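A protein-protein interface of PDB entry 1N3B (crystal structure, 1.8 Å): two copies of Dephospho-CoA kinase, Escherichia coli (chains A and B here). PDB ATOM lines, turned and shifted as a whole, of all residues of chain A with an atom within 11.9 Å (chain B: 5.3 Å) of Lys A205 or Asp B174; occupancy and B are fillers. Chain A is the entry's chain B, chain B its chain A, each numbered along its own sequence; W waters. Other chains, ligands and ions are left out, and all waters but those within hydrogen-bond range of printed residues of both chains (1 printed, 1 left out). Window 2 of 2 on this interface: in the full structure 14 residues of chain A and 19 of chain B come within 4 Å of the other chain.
NH1 of Arg B162 lies within hydrogen-bond range of O of Gln A203 (2.7 Å).
The guanidinium group (NH2) of Arg B162 lies within hydrogen-bond range of the backbone carbonyl oxygen (O) of Glu A204 (2.9 Å).
The side-chain amide nitrogen (ND2) of Asn B176 lies within hydrogen-bond range of the backbone carbonyl oxygen (O) of Glu A204 (2.9 Å).
NH2 of Arg B162 is in salt-bridge range of OD1 of Asp B131, at 2.7 Å.
The backbone NH of Asp B131 is in hydrogen-bond range of the backbone carbonyl oxygen of Ile B173, at 2.8 Å.
O of Asp B131 sits at hydrogen-bond distance from N of Asn B175.
The backbone carbonyl oxygen (O) of Val B132 sits at hydrogen-bond distance from the guanidinium group (NE) of Arg B162 (3.3 Å).
The side-chain amide nitrogen (NE2) of Gln A199 sits at hydrogen-bond distance from the side-chain amide oxygen (OE1) of Gln A203 (2.6 Å).
NE2 of Gln A203 lies within hydrogen-bond range of O of Lys A205 (3.0 Å).
Asp B131 touches Glu A204.
Glu A204 touches Asp B174 (O to OD2, 3.6 Å).
C of Lys A205 touches NH2 of Arg B162, at 3.9 Å.
CG of Lys A205 touches OD2 of Asp B174, at 3.5 Å.
CG of Pro A206 touches OD1 of Asp B131, 3.4 Å away.
Pro A206 touches Arg B162 (N to NH2, 3.9 Å).
Ser A202 touches none of the printed residues of chain B.
Of the printed residues of chain B, Gln A203 touches Arg B162.
Printed residues of chain B within 4 Å of Glu A204: Asp B131, Arg B162, Asp B174 and Asn B176.
Of chain B, only Arg B162 (3.9 Å) and Asp B174 (3.5 Å) come within 4 Å of Lys A205.
Printed residues of chain B within 4 Å of Pro A206: Asp B131 (3.4 Å) and Arg B162 (3.9 Å).
No residue of chain A comes within 4 Å of Val B132.
Of the printed residues of chain A, Arg B162 touches Gln A203, Glu A204, Lys A205 and Pro A206.
No residue of chain A comes within 4 Å of Val B172.
No residue of chain A comes within 4 Å of Ile B173.
Asp B174 touches two residues of chain A.
Asn B176 touches just one residue of chain A: Glu A204 (2.9 Å).
No residue of chain A comes within 4 Å of Ile B182.
Asp B185 touches none of the printed residues of chain A.
The nearest residue of chain A that does not touch Asp B174 is Pro A206 (6.0 Å).
Hydrophobic or aromatic side chains of chain A within 4 Å of the printed part of chain B: Pro A206.
Among the printed residues, 9 pairs touch across the chains.
No position is printed for both chains.
Of the 9 pairs that touch across the chains among the printed residues, none has its exchanged pair printed and touching as well.
Water W1 bridges the backbone carbonyl oxygen (O) of Phe A200 (2.6 Å) and the guanidinium group (NH1) of Arg B162 (2.9 Å).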
ATOM      1  N   TYR A   3      40.658  -5.828 -10.210  1.00  0.00           N
ATOM      2  CA  TYR A   3      40.505  -4.877 -11.302  1.00  0.00           C
ATOM      3  C   TYR A   3      41.859  -4.812 -12.007  1.00  0.00           C
ATOM      4  O   TYR A   3      42.897  -4.771 -11.344  1.00  0.00           O
ATOM      5  CB  TYR A   3      40.131  -3.517 -10.714  1.00  0.00           C
ATOM      6  CG  TYR A   3      39.635  -2.527 -11.724  1.00  0.00           C
ATOM      7  CD1 TYR A   3      38.370  -2.658 -12.289  1.00  0.00           C
ATOM      8  CD2 TYR A   3      40.426  -1.448 -12.105  1.00  0.00           C
ATOM      9  CE1 TYR A   3      37.903  -1.736 -13.217  1.00  0.00           C
ATOM     10  CE2 TYR A   3      39.970  -0.508 -13.021  1.00  0.00           C
ATOM     11  CZ  TYR A   3      38.712  -0.664 -13.576  1.00  0.00           C
ATOM     12  OH  TYR A   3      38.261   0.248 -14.499  1.00  0.00           O
ATOM     13  N   ARG A 126      40.814  -1.359 -17.755  1.00  0.00           N
ATOM     14  CA  ARG A 126      41.147   0.044 -17.964  1.00  0.00           C
ATOM     15  C   ARG A 126      42.531   0.110 -18.601  1.00  0.00           C
ATOM     16  O   ARG A 126      43.389  -0.697 -18.280  1.00  0.00           O
ATOM     17  CB  ARG A 126      41.165   0.732 -16.601  1.00  0.00           C
ATOM     18  CG  ARG A 126      41.367   2.244 -16.623  1.00  0.00           C
ATOM     19  CD  ARG A 126      40.030   2.932 -16.660  1.00  0.00           C
ATOM     20  NE  ARG A 126      40.146   4.385 -16.544  1.00  0.00           N
ATOM     21  CZ  ARG A 126      39.099   5.196 -16.584  1.00  0.00           C
ATOM     22  NH1 ARG A 126      37.884   4.683 -16.721  1.00  0.00           N
ATOM     23  NH2 ARG A 126      39.260   6.511 -16.522  1.00  0.00           N
ATOM     24  N   GLN A 195      38.596   3.673  -6.607  1.00  0.00           N
ATOM     25  CA  GLN A 195      37.141   3.855  -6.674  1.00  0.00           C
ATOM     26  C   GLN A 195      36.541   2.859  -7.672  1.00  0.00           C
ATOM     27  O   GLN A 195      35.547   2.177  -7.377  1.00  0.00           O
ATOM     28  CB  GLN A 195      36.792   5.280  -7.103  1.00  0.00           C
ATOM     29  CG  GLN A 195      35.301   5.497  -7.343  1.00  0.00           C
ATOM     30  CD  GLN A 195      34.470   5.276  -6.100  1.00  0.00           C
ATOM     31  OE1 GLN A 195      34.677   5.933  -5.081  1.00  0.00           O
ATOM     32  NE2 GLN A 195      33.514   4.355  -6.176  1.00  0.00           N
ATOM     33  N   LEU A 196      37.148   2.767  -8.862  1.00  0.00           N
ATOM     34  CA  LEU A 196      36.643   1.835  -9.870  1.00  0.00           C
ATOM     35  C   LEU A 196      36.755   0.403  -9.368  1.00  0.00           C
ATOM     36  O   LEU A 196      35.858  -0.420  -9.566  1.00  0.00           O
ATOM     37  CB  LEU A 196      37.424   2.013 -11.183  1.00  0.00           C
ATOM     38  CG  LEU A 196      37.259   3.391 -11.850  1.00  0.00           C
ATOM     39  CD1 LEU A 196      38.319   3.603 -12.939  1.00  0.00           C
ATOM     40  CD2 LEU A 196      35.837   3.494 -12.456  1.00  0.00           C
ATOM     41  N   SER A 198      36.621  -0.591  -6.326  1.00  0.00           N
ATOM     42  CA  SER A 198      35.670  -0.830  -5.250  1.00  0.00           C
ATOM     43  C   SER A 198      34.252  -1.104  -5.734  1.00  0.00           C
ATOM     44  O   SER A 198      33.473  -1.766  -5.049  1.00  0.00           O
ATOM     45  CB  SER A 198      35.640   0.364  -4.296  1.00  0.00           C
ATOM     46  OG  SER A 198      34.829   1.397  -4.838  1.00  0.00           O
ATOM     47  N   GLN A 199      33.929  -0.629  -6.934  1.00  0.00           N
ATOM     48  CA  GLN A 199      32.566  -0.750  -7.451  1.00  0.00           C
ATOM     49  C   GLN A 199      32.335  -1.703  -8.607  1.00  0.00           C
ATOM     50  O   GLN A 199      31.211  -2.162  -8.833  1.00  0.00           O
ATOM     51  CB  GLN A 199      32.111   0.642  -7.918  1.00  0.00           C
ATOM     52  CG  GLN A 199      32.884   1.094  -9.176  1.00  0.00           C
ATOM     53  CD  GLN A 199      32.580   2.537  -9.620  1.00  0.00           C
ATOM     54  OE1 GLN A 199      32.655   3.474  -8.820  1.00  0.00           O
ATOM     55  NE2 GLN A 199      32.275   2.715 -10.908  1.00  0.00           N
ATOM     56  N   PHE A 200      33.396  -2.009  -9.341  1.00  0.00           N
ATOM     57  CA  PHE A 200      33.250  -2.800 -10.556  1.00  0.00           C
ATOM     58  C   PHE A 200      32.580  -4.177 -10.534  1.00  0.00           C
ATOM     59  O   PHE A 200      31.847  -4.519 -11.482  1.00  0.00           O
ATOM     60  CB  PHE A 200      34.606  -2.831 -11.306  1.00  0.00           C
ATOM     61  CG  PHE A 200      35.445  -4.049 -11.037  1.00  0.00           C
ATOM     62  CD1 PHE A 200      35.521  -5.074 -11.984  1.00  0.00           C
ATOM     63  CD2 PHE A 200      36.171  -4.168  -9.859  1.00  0.00           C
ATOM     64  CE1 PHE A 200      36.311  -6.203 -11.764  1.00  0.00           C
ATOM     65  CE2 PHE A 200      36.965  -5.297  -9.626  1.00  0.00           C
ATOM     66  CZ  PHE A 200      37.033  -6.312 -10.584  1.00  0.00           C
ATOM     67  N   VAL A 201      32.767  -4.967  -9.482  1.00  0.00           N
ATOM     68  CA  VAL A 201      32.146  -6.287  -9.486  1.00  0.00           C
ATOM     69  C   VAL A 201      30.612  -6.249  -9.491  1.00  0.00           C
ATOM     70  O   VAL A 201      29.981  -6.953 -10.267  1.00  0.00           O
ATOM     71  CB  VAL A 201      32.670  -7.152  -8.307  1.00  0.00           C
ATOM     72  CG1 VAL A 201      31.887  -8.458  -8.208  1.00  0.00           C
ATOM     73  CG2 VAL A 201      34.142  -7.479  -8.543  1.00  0.00           C
ATOM     74  N   SER A 202      30.024  -5.406  -8.650  1.00  0.00           N
ATOM     75  CA  SER A 202      28.566  -5.302  -8.563  1.00  0.00           C
ATOM     76  C   SER A 202      27.932  -4.145  -9.327  1.00  0.00           C
ATOM     77  O   SER A 202      26.722  -3.965  -9.258  1.00  0.00           O
ATOM     78  CB  SER A 202      28.157  -5.196  -7.091  1.00  0.00           C
ATOM     79  OG  SER A 202      28.568  -6.349  -6.381  1.00  0.00           O
ATOM     80  N   GLN A 203      28.726  -3.353 -10.046  1.00  0.00           N
ATOM     81  CA  GLN A 203      28.192  -2.203 -10.790  1.00  0.00           C
ATOM     82  C   GLN A 203      27.139  -2.652 -11.817  1.00  0.00           C
ATOM     83  O   GLN A 203      27.464  -3.340 -12.778  1.00  0.00           O
ATOM     84  CB  GLN A 203      29.347  -1.490 -11.495  1.00  0.00           C
ATOM     85  CG  GLN A 203      29.066  -0.078 -11.997  1.00  0.00           C
ATOM     86  CD  GLN A 203      30.302   0.534 -12.646  1.00  0.00           C
ATOM     87  OE1 GLN A 203      31.392   0.510 -12.079  1.00  0.00           O
ATOM     88  NE2 GLN A 203      30.136   1.083 -13.835  1.00  0.00           N
ATOM     89  N   GLU A 204      25.878  -2.258 -11.643  1.00  0.00           N
ATOM     90  CA  GLU A 204      24.864  -2.719 -12.594  1.00  0.00           C
ATOM     91  C   GLU A 204      24.923  -2.086 -13.968  1.00  0.00           C
ATOM     92  O   GLU A 204      24.769  -2.782 -14.983  1.00  0.00           O
ATOM     93  CB  GLU A 204      23.458  -2.577 -12.017  1.00  0.00           C
ATOM     94  CG  GLU A 204      23.089  -3.744 -11.104  1.00  0.00           C
ATOM     95  CD  GLU A 204      21.600  -3.851 -10.848  1.00  0.00           C
ATOM     96  OE1 GLU A 204      20.848  -4.118 -11.810  1.00  0.00           O
ATOM     97  OE2 GLU A 204      21.185  -3.675  -9.684  1.00  0.00           O
ATOM     98  N   LYS A 205      25.147  -0.779 -14.013  1.00  0.00           N
ATOM     99  CA  LYS A 205      25.219  -0.094 -15.289  1.00  0.00           C
ATOM    100  C   LYS A 205      26.598   0.522 -15.535  1.00  0.00           C
ATOM    101  O   LYS A 205      27.261   0.984 -14.604  1.00  0.00           O
ATOM    102  CB  LYS A 205      24.105   0.953 -15.380  1.00  0.00           C
ATOM    103  CG  LYS A 205      22.708   0.311 -15.493  1.00  0.00           C
ATOM    104  CD  LYS A 205      21.618   1.343 -15.754  1.00  0.00           C
ATOM    105  CE  LYS A 205      21.096   1.965 -14.472  1.00  0.00           C
ATOM    106  NZ  LYS A 205      20.292   0.978 -13.684  1.00  0.00           N
ATOM    107  N   PRO A 206      27.046   0.522 -16.802  1.00  0.00           N
ATOM    108  CA  PRO A 206      28.349   1.066 -17.206  1.00  0.00           C
ATOM    109  C   PRO A 206      28.519   2.514 -16.790  1.00  0.00           C
ATOM    110  O   PRO A 206      27.481   3.178 -16.590  1.00  0.00           O
ATOM    111  CB  PRO A 206      28.332   0.929 -18.729  1.00  0.00           C
ATOM    112  CG  PRO A 206      27.386  -0.207 -18.973  1.00  0.00           C
ATOM    113  CD  PRO A 206      26.282   0.067 -17.978  1.00  0.00           C
ATOM    114  N   ASP B 131      24.747  -6.349 -21.665  1.00  0.00           N
ATOM    115  CA  ASP B 131      25.598  -6.051 -20.525  1.00  0.00           C
ATOM    116  C   ASP B 131      25.034  -6.418 -19.151  1.00  0.00           C
ATOM    117  O   ASP B 131      23.838  -6.248 -18.889  1.00  0.00           O
ATOM    118  CB  ASP B 131      25.922  -4.556 -20.567  1.00  0.00           C
ATOM    119  CG  ASP B 131      26.847  -4.124 -19.466  1.00  0.00           C
ATOM    120  OD1 ASP B 131      26.391  -3.398 -18.556  1.00  0.00           O
ATOM    121  OD2 ASP B 131      28.025  -4.513 -19.506  1.00  0.00           O
ATOM    122  N   VAL B 132      25.919  -6.918 -18.292  1.00  0.00           N
ATOM    123  CA  VAL B 132      25.582  -7.266 -16.916  1.00  0.00           C
ATOM    124  C   VAL B 132      26.816  -7.030 -16.045  1.00  0.00           C
ATOM    125  O   VAL B 132      27.923  -6.830 -16.552  1.00  0.00           O
ATOM    126  CB  VAL B 132      25.120  -8.741 -16.767  1.00  0.00           C
ATOM    127  CG1 VAL B 132      23.836  -8.965 -17.587  1.00  0.00           C
ATOM    128  CG2 VAL B 132      26.234  -9.705 -17.209  1.00  0.00           C
ATOM    129  N   ARG B 162      34.380  -6.611 -19.602  1.00  0.00           N
ATOM    130  CA  ARG B 162      33.141  -5.868 -19.789  1.00  0.00           C
ATOM    131  C   ARG B 162      33.434  -4.578 -20.554  1.00  0.00           C
ATOM    132  O   ARG B 162      32.729  -4.237 -21.496  1.00  0.00           O
ATOM    133  CB  ARG B 162      32.542  -5.511 -18.428  1.00  0.00           C
ATOM    134  CG  ARG B 162      31.254  -4.672 -18.495  1.00  0.00           C
ATOM    135  CD  ARG B 162      30.782  -4.302 -17.095  1.00  0.00           C
ATOM    136  NE  ARG B 162      29.374  -3.890 -17.084  1.00  0.00           N
ATOM    137  CZ  ARG B 162      28.696  -3.608 -15.970  1.00  0.00           C
ATOM    138  NH1 ARG B 162      29.300  -3.688 -14.789  1.00  0.00           N
ATOM    139  NH2 ARG B 162      27.411  -3.268 -16.025  1.00  0.00           N
ATOM    140  N   VAL B 172      23.791  -0.779 -26.083  1.00  0.00           N
ATOM    141  CA  VAL B 172      23.998  -1.598 -24.891  1.00  0.00           C
ATOM    142  C   VAL B 172      22.653  -1.872 -24.249  1.00  0.00           C
ATOM    143  O   VAL B 172      21.823  -0.965 -24.106  1.00  0.00           O
ATOM    144  CB  VAL B 172      24.882  -0.878 -23.835  1.00  0.00           C
ATOM    145  CG1 VAL B 172      25.074  -1.790 -22.615  1.00  0.00           C
ATOM    146  CG2 VAL B 172      26.248  -0.504 -24.437  1.00  0.00           C
ATOM    147  N   ILE B 173      22.426  -3.123 -23.875  1.00  0.00           N
ATOM    148  CA  ILE B 173      21.174  -3.486 -23.217  1.00  0.00           C
ATOM    149  C   ILE B 173      21.500  -4.199 -21.896  1.00  0.00           C
ATOM    150  O   ILE B 173      22.222  -5.203 -21.866  1.00  0.00           O
ATOM    151  CB  ILE B 173      20.286  -4.350 -24.155  1.00  0.00           C
ATOM    152  CG1 ILE B 173      18.948  -4.672 -23.467  1.00  0.00           C
ATOM    153  CG2 ILE B 173      21.042  -5.613 -24.588  1.00  0.00           C
ATOM    154  CD1 ILE B 173      17.907  -5.333 -24.406  1.00  0.00           C
ATOM    155  N   ASP B 174      21.012  -3.625 -20.801  1.00  0.00           N
ATOM    156  CA  ASP B 174      21.220  -4.168 -19.451  1.00  0.00           C
ATOM    157  C   ASP B 174      20.388  -5.434 -19.284  1.00  0.00           C
ATOM    158  O   ASP B 174      19.182  -5.414 -19.532  1.00  0.00           O
ATOM    159  CB  ASP B 174      20.764  -3.131 -18.412  1.00  0.00           C
ATOM    160  CG  ASP B 174      20.921  -3.610 -16.962  1.00  0.00           C
ATOM    161  OD1 ASP B 174      20.615  -4.775 -16.654  1.00  0.00           O
ATOM    162  OD2 ASP B 174      21.327  -2.790 -16.119  1.00  0.00           O
ATOM    163  N   ASN B 175      21.005  -6.536 -18.873  1.00  0.00           N
ATOM    164  CA  ASN B 175      20.224  -7.754 -18.679  1.00  0.00           C
ATOM    165  C   ASN B 175      20.487  -8.338 -17.291  1.00  0.00           C
ATOM    166  O   ASN B 175      20.546  -9.560 -17.125  1.00  0.00           O
ATOM    167  CB  ASN B 175      20.532  -8.813 -19.743  1.00  0.00           C
ATOM    168  CG  ASN B 175      19.551  -9.989 -19.691  1.00  0.00           C
ATOM    169  OD1 ASN B 175      19.881 -11.129 -20.040  1.00  0.00           O
ATOM    170  ND2 ASN B 175      18.335  -9.708 -19.256  1.00  0.00           N
ATOM    171  N   ASN B 176      20.644  -7.452 -16.309  1.00  0.00           N
ATOM    172  CA  ASN B 176      20.883  -7.860 -14.922  1.00  0.00           C
ATOM    173  C   ASN B 176      19.652  -8.463 -14.242  1.00  0.00           C
ATOM    174  O   ASN B 176      19.780  -9.306 -13.341  1.00  0.00           O
ATOM    175  CB  ASN B 176      21.338  -6.670 -14.092  1.00  0.00           C
ATOM    176  CG  ASN B 176      22.791  -6.338 -14.307  1.00  0.00           C
ATOM    177  OD1 ASN B 176      23.677  -7.143 -13.998  1.00  0.00           O
ATOM    178  ND2 ASN B 176      23.047  -5.152 -14.843  1.00  0.00           N
ATOM    179  N   GLY B 177      18.467  -8.023 -14.668  1.00  0.00           N
ATOM    180  CA  GLY B 177      17.238  -8.508 -14.056  1.00  0.00           C
ATOM    181  C   GLY B 177      16.518  -9.656 -14.739  1.00  0.00           C
ATOM    182  O   GLY B 177      17.131 -10.516 -15.376  1.00  0.00           O
ATOM    183  N   ILE B 182      13.792  -6.313 -20.120  1.00  0.00           N
ATOM    184  CA  ILE B 182      14.447  -5.814 -21.327  1.00  0.00           C
ATOM    185  C   ILE B 182      13.470  -5.333 -22.412  1.00  0.00           C
ATOM    186  O   ILE B 182      13.896  -4.748 -23.408  1.00  0.00           O
ATOM    187  CB  ILE B 182      15.355  -6.901 -21.976  1.00  0.00           C
ATOM    188  CG1 ILE B 182      14.503  -8.011 -22.602  1.00  0.00           C
ATOM    189  CG2 ILE B 182      16.283  -7.514 -20.923  1.00  0.00           C
ATOM    190  CD1 ILE B 182      15.298  -8.938 -23.502  1.00  0.00           C
ATOM    191  N   ASP B 185      13.813  -1.728 -23.905  1.00  0.00           N
ATOM    192  CA  ASP B 185      15.006  -1.553 -24.751  1.00  0.00           C
ATOM    193  C   ASP B 185      14.874  -2.315 -26.067  1.00  0.00           C
ATOM    194  O   ASP B 185      15.248  -1.811 -27.122  1.00  0.00           O
ATOM    195  CB  ASP B 185      16.279  -2.040 -24.040  1.00  0.00           C
ATOM    196  CG  ASP B 185      16.725  -1.123 -22.916  1.00  0.00           C
ATOM    197  OD1 ASP B 185      16.616   0.114 -23.059  1.00  0.00           O
ATOM    198  OD2 ASP B 185      17.211  -1.643 -21.892  1.00  0.00           O
HETATM  199  O   HOH W   1      32.104  -3.677 -13.974  1.00  0.00           O
